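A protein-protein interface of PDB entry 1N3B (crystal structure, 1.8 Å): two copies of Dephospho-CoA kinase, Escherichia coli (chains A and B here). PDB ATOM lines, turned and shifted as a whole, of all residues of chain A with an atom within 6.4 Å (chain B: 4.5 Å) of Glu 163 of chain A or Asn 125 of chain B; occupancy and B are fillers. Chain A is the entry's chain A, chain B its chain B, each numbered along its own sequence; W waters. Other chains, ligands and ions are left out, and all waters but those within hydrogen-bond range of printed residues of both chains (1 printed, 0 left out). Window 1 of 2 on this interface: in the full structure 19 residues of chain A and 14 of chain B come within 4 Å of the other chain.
Of chain B, only Asn 125 (3.0 Å) comes within 4 Å of Glu 163 of chain A.
Of chain A, only Thr 161 (3.7 Å) and Glu 163 (3.0 Å) come within 4 Å of Asn 125 of chain B.
Of the printed residues of chain A, Lys 123 of chain B touches Thr 161 (3.5 Å).
Of the printed residues of chain B, Thr 161 of chain A touches Lys 123 (3.5 Å), Ala 124 (2.8 Å) and Asn 125 (3.7 Å).
Printed residues of chain A within 4 Å of Ala 124 of chain B: Thr 161 (2.8 Å).
Arg 2 of chain B touches none of the printed residues of chain A.
Among the printed residues, 4 pairs touch across the chains.
Among the printed residues, no Asp or Glu carboxylate lies within 4 Å of a Lys or Arg side-chain nitrogen of the other chain.
The side-chain hydroxyl (OG1) of Thr 161 of chain A lies within hydrogen-bond range of the backbone carbonyl oxygen (O) of Ala 124 of chain B, 2.8 Å away.
The side-chain amide oxygen of Asn 125 of chain B lies close to the side-chain carboxylate of Glu 163 of chain A (3.0 Å).
Water W1 lies within hydrogen-bond range of the side-chain hydroxyl (OH) of Tyr 3 of chain B (2.6 Å) and the side-chain carboxylate (OE2) of Glu 163 of chain A (2.8 Å).
CG2 of Thr 161 of chain A touches C of Lys 123 of chain B, 3.5 Å away.
Thr 161 of chain A touches Asn 125 of chain B.
The backbone NH (N) of Ala 164 of chain A is in hydrogen-bond range of the side-chain hydroxyl (OG1) of Thr 161 of chain A, 3.1 Å away.
N of Ile 4 of chain B sits close to ND2 of Asn 125 of chain B, 2.8 Å away.
No position is printed for both chains.
Of the 4 pairs that touch across the chains among the printed residues, none has its exchanged pair printed and touching as well.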
ATOM      1  N   ALA A 160      -3.088  -1.126  -8.474  1.00  0.00           N
ATOM      2  CA  ALA A 160      -3.174  -2.500  -8.932  1.00  0.00           C
ATOM      3  C   ALA A 160      -4.539  -3.025  -8.525  1.00  0.00           C
ATOM      4  O   ALA A 160      -5.174  -2.492  -7.600  1.00  0.00           O
ATOM      5  CB  ALA A 160      -2.066  -3.350  -8.288  1.00  0.00           C
ATOM      6  N   THR A 161      -4.991  -4.072  -9.210  1.00  0.00           N
ATOM      7  CA  THR A 161      -6.280  -4.666  -8.916  1.00  0.00           C
ATOM      8  C   THR A 161      -6.196  -5.607  -7.724  1.00  0.00           C
ATOM      9  O   THR A 161      -5.113  -6.018  -7.292  1.00  0.00           O
ATOM     10  CB  THR A 161      -6.814  -5.482 -10.103  1.00  0.00           C
ATOM     11  OG1 THR A 161      -5.908  -6.558 -10.377  1.00  0.00           O
ATOM     12  CG2 THR A 161      -6.946  -4.610 -11.352  1.00  0.00           C
ATOM     13  N   ARG A 162      -7.363  -5.958  -7.201  1.00  0.00           N
ATOM     14  CA  ARG A 162      -7.440  -6.870  -6.069  1.00  0.00           C
ATOM     15  C   ARG A 162      -6.737  -8.180  -6.424  1.00  0.00           C
ATOM     16  O   ARG A 162      -5.953  -8.700  -5.640  1.00  0.00           O
ATOM     17  CB  ARG A 162      -8.904  -7.168  -5.743  1.00  0.00           C
ATOM     18  CG  ARG A 162      -9.114  -8.170  -4.594  1.00  0.00           C
ATOM     19  CD  ARG A 162     -10.597  -8.460  -4.401  1.00  0.00           C
ATOM     20  NE  ARG A 162     -10.871  -9.049  -3.086  1.00  0.00           N
ATOM     21  CZ  ARG A 162     -12.100  -9.307  -2.635  1.00  0.00           C
ATOM     22  NH1 ARG A 162     -13.155  -9.034  -3.394  1.00  0.00           N
ATOM     23  NH2 ARG A 162     -12.284  -9.816  -1.418  1.00  0.00           N
ATOM     24  N   GLU A 163      -7.030  -8.706  -7.612  1.00  0.00           N
ATOM     25  CA  GLU A 163      -6.439  -9.976  -8.037  1.00  0.00           C
ATOM     26  C   GLU A 163      -4.925  -9.893  -8.247  1.00  0.00           C
ATOM     27  O   GLU A 163      -4.211 -10.869  -8.051  1.00  0.00           O
ATOM     28  CB  GLU A 163      -7.129 -10.486  -9.316  1.00  0.00           C
ATOM     29  CG  GLU A 163      -8.652 -10.712  -9.179  1.00  0.00           C
ATOM     30  CD  GLU A 163      -9.492  -9.428  -9.308  1.00  0.00           C
ATOM     31  OE1 GLU A 163      -8.929  -8.312  -9.459  1.00  0.00           O
ATOM     32  OE2 GLU A 163     -10.732  -9.551  -9.259  1.00  0.00           O
ATOM     33  N   ALA A 164      -4.435  -8.732  -8.653  1.00  0.00           N
ATOM     34  CA  ALA A 164      -3.001  -8.555  -8.854  1.00  0.00           C
ATOM     35  C   ALA A 164      -2.293  -8.607  -7.493  1.00  0.00           C
ATOM     36  O   ALA A 164      -1.162  -9.117  -7.377  1.00  0.00           O
ATOM     37  CB  ALA A 164      -2.732  -7.226  -9.557  1.00  0.00           C
ATOM     38  N   ARG A 165      -2.946  -8.088  -6.457  1.00  0.00           N
ATOM     39  CA  ARG A 165      -2.349  -8.145  -5.127  1.00  0.00           C
ATOM     40  C   ARG A 165      -2.384  -9.583  -4.606  1.00  0.00           C
ATOM     41  O   ARG A 165      -1.417 -10.050  -4.014  1.00  0.00           O
ATOM     42  CB  ARG A 165      -3.088  -7.229  -4.135  1.00  0.00           C
ATOM     43  CG  ARG A 165      -2.795  -5.737  -4.352  1.00  0.00           C
ATOM     44  CD  ARG A 165      -3.367  -4.898  -3.240  1.00  0.00           C
ATOM     45  NE  ARG A 165      -4.825  -5.008  -3.245  1.00  0.00           N
ATOM     46  CZ  ARG A 165      -5.630  -4.141  -3.853  1.00  0.00           C
ATOM     47  NH1 ARG A 165      -5.113  -3.103  -4.486  1.00  0.00           N
ATOM     48  NH2 ARG A 165      -6.944  -4.331  -3.849  1.00  0.00           N
ATOM     49  N   LEU A 166      -3.492 -10.277  -4.847  1.00  0.00           N
ATOM     50  CA  LEU A 166      -3.633 -11.652  -4.382  1.00  0.00           C
ATOM     51  C   LEU A 166      -2.595 -12.550  -5.050  1.00  0.00           C
ATOM     52  O   LEU A 166      -2.111 -13.501  -4.437  1.00  0.00           O
ATOM     53  CB  LEU A 166      -5.065 -12.183  -4.658  1.00  0.00           C
ATOM     54  CG  LEU A 166      -6.220 -11.474  -3.903  1.00  0.00           C
ATOM     55  CD1 LEU A 166      -7.615 -12.015  -4.340  1.00  0.00           C
ATOM     56  CD2 LEU A 166      -6.027 -11.675  -2.399  1.00  0.00           C
ATOM     57  N   ALA A 167      -2.240 -12.238  -6.295  1.00  0.00           N
ATOM     58  CA  ALA A 167      -1.260 -13.041  -7.033  1.00  0.00           C
ATOM     59  C   ALA A 167       0.112 -13.060  -6.408  1.00  0.00           C
ATOM     60  O   ALA A 167       0.857 -14.003  -6.623  1.00  0.00           O
ATOM     61  CB  ALA A 167      -1.136 -12.562  -8.499  1.00  0.00           C
ATOM     62  N   VAL A 168       0.465 -12.026  -5.652  1.00  0.00           N
ATOM     63  CA  VAL A 168       1.784 -12.012  -5.027  1.00  0.00           C
ATOM     64  C   VAL A 168       1.738 -12.234  -3.525  1.00  0.00           C
ATOM     65  O   VAL A 168       2.778 -12.239  -2.877  1.00  0.00           O
ATOM     66  CB  VAL A 168       2.521 -10.687  -5.310  1.00  0.00           C
ATOM     67  CG1 VAL A 168       2.676 -10.495  -6.799  1.00  0.00           C
ATOM     68  CG2 VAL A 168       1.777  -9.528  -4.670  1.00  0.00           C
ATOM     69  N   ARG B   2     -16.333  -1.631 -14.039  1.00  0.00           N
ATOM     70  CA  ARG B   2     -16.443  -2.741 -14.958  1.00  0.00           C
ATOM     71  C   ARG B   2     -15.307  -3.717 -14.739  1.00  0.00           C
ATOM     72  O   ARG B   2     -14.187  -3.329 -14.423  1.00  0.00           O
ATOM     73  CB  ARG B   2     -16.450  -2.231 -16.405  1.00  0.00           C
ATOM     74  CG  ARG B   2     -17.817  -2.365 -17.056  1.00  0.00           C
ATOM     75  CD  ARG B   2     -18.239  -1.103 -17.781  1.00  0.00           C
ATOM     76  NE  ARG B   2     -19.681  -1.085 -18.033  1.00  0.00           N
ATOM     77  CZ  ARG B   2     -20.612  -1.006 -17.085  1.00  0.00           C
ATOM     78  NH1 ARG B   2     -20.265  -0.941 -15.807  1.00  0.00           N
ATOM     79  NH2 ARG B   2     -21.899  -0.976 -17.413  1.00  0.00           N
ATOM     80  N   TYR B   3     -15.622  -4.995 -14.890  1.00  0.00           N
ATOM     81  CA  TYR B   3     -14.645  -6.060 -14.711  1.00  0.00           C
ATOM     82  C   TYR B   3     -13.733  -6.016 -15.935  1.00  0.00           C
ATOM     83  O   TYR B   3     -14.216  -5.857 -17.058  1.00  0.00           O
ATOM     84  CB  TYR B   3     -15.387  -7.393 -14.631  1.00  0.00           C
ATOM     85  CG  TYR B   3     -14.550  -8.533 -14.135  1.00  0.00           C
ATOM     86  CD1 TYR B   3     -14.194  -8.624 -12.792  1.00  0.00           C
ATOM     87  CD2 TYR B   3     -14.127  -9.532 -15.005  1.00  0.00           C
ATOM     88  CE1 TYR B   3     -13.428  -9.685 -12.327  1.00  0.00           C
ATOM     89  CE2 TYR B   3     -13.372 -10.608 -14.554  1.00  0.00           C
ATOM     90  CZ  TYR B   3     -13.022 -10.673 -13.218  1.00  0.00           C
ATOM     91  OH  TYR B   3     -12.258 -11.721 -12.767  1.00  0.00           O
ATOM     92  N   ILE B   4     -12.426  -6.140 -15.715  1.00  0.00           N
ATOM     93  CA  ILE B   4     -11.453  -6.064 -16.801  1.00  0.00           C
ATOM     94  C   ILE B   4     -10.746  -7.389 -17.039  1.00  0.00           C
ATOM     95  O   ILE B   4     -10.034  -7.886 -16.180  1.00  0.00           O
ATOM     96  CB  ILE B   4     -10.351  -5.005 -16.484  1.00  0.00           C
ATOM     97  CG1 ILE B   4     -11.002  -3.646 -16.231  1.00  0.00           C
ATOM     98  CG2 ILE B   4      -9.318  -4.938 -17.630  1.00  0.00           C
ATOM     99  CD1 ILE B   4     -10.030  -2.598 -15.637  1.00  0.00           C
ATOM    100  N   LYS B 123      -2.968  -4.430 -13.870  1.00  0.00           N
ATOM    101  CA  LYS B 123      -4.153  -3.581 -13.984  1.00  0.00           C
ATOM    102  C   LYS B 123      -5.385  -4.346 -14.478  1.00  0.00           C
ATOM    103  O   LYS B 123      -6.411  -3.734 -14.816  1.00  0.00           O
ATOM    104  CB  LYS B 123      -3.901  -2.411 -14.949  1.00  0.00           C
ATOM    105  CG  LYS B 123      -2.588  -1.665 -14.730  1.00  0.00           C
ATOM    106  CD  LYS B 123      -2.443  -1.183 -13.284  1.00  0.00           C
ATOM    107  CE  LYS B 123      -3.591  -0.267 -12.858  1.00  0.00           C
ATOM    108  NZ  LYS B 123      -4.831  -1.016 -12.514  1.00  0.00           N
ATOM    109  N   ALA B 124      -5.284  -5.665 -14.574  1.00  0.00           N
ATOM    110  CA  ALA B 124      -6.440  -6.457 -15.023  1.00  0.00           C
ATOM    111  C   ALA B 124      -7.000  -7.280 -13.857  1.00  0.00           C
ATOM    112  O   ALA B 124      -6.279  -7.625 -12.925  1.00  0.00           O
ATOM    113  CB  ALA B 124      -6.039  -7.395 -16.155  1.00  0.00           C
ATOM    114  N   ASN B 125      -8.295  -7.598 -13.914  1.00  0.00           N
ATOM    115  CA  ASN B 125      -8.899  -8.416 -12.865  1.00  0.00           C
ATOM    116  C   ASN B 125      -8.717  -9.876 -13.247  1.00  0.00           C
ATOM    117  O   ASN B 125      -8.721 -10.761 -12.396  1.00  0.00           O
ATOM    118  CB  ASN B 125     -10.396  -8.113 -12.730  1.00  0.00           C
ATOM    119  CG  ASN B 125     -10.657  -6.698 -12.277  1.00  0.00           C
ATOM    120  OD1 ASN B 125     -10.303  -6.317 -11.161  1.00  0.00           O
ATOM    121  ND2 ASN B 125     -11.269  -5.909 -13.143  1.00  0.00           N
ATOM    122  N   ARG B 126      -8.513 -10.120 -14.532  1.00  0.00           N
ATOM    123  CA  ARG B 126      -8.359 -11.482 -15.028  1.00  0.00           C
ATOM    124  C   ARG B 126      -7.508 -11.429 -16.293  1.00  0.00           C
ATOM    125  O   ARG B 126      -7.622 -10.489 -17.065  1.00  0.00           O
ATOM    126  CB  ARG B 126      -9.748 -12.025 -15.354  1.00  0.00           C
ATOM    127  CG  ARG B 126      -9.806 -13.493 -15.766  1.00  0.00           C
ATOM    128  CD  ARG B 126     -10.043 -14.350 -14.552  1.00  0.00           C
ATOM    129  NE  ARG B 126     -10.248 -15.756 -14.894  1.00  0.00           N
ATOM    130  CZ  ARG B 126     -10.443 -16.697 -13.981  1.00  0.00           C
ATOM    131  NH1 ARG B 126     -10.470 -16.363 -12.698  1.00  0.00           N
ATOM    132  NH2 ARG B 126     -10.575 -17.968 -14.337  1.00  0.00           N
ATOM    133  N   ASP B 170      -4.710 -16.488 -16.180  1.00  0.00           N
ATOM    134  CA  ASP B 170      -5.739 -17.107 -15.348  1.00  0.00           C
ATOM    135  C   ASP B 170      -6.412 -18.147 -16.235  1.00  0.00           C
ATOM    136  O   ASP B 170      -6.740 -19.237 -15.769  1.00  0.00           O
ATOM    137  CB  ASP B 170      -6.768 -16.085 -14.898  1.00  0.00           C
ATOM    138  CG  ASP B 170      -6.187 -15.113 -13.915  1.00  0.00           C
ATOM    139  OD1 ASP B 170      -5.751 -15.588 -12.837  1.00  0.00           O
ATOM    140  OD2 ASP B 170      -6.150 -13.901 -14.218  1.00  0.00           O
HETATM  141  O   HOH W   1     -12.000 -11.839 -10.143  1.00  0.00           O
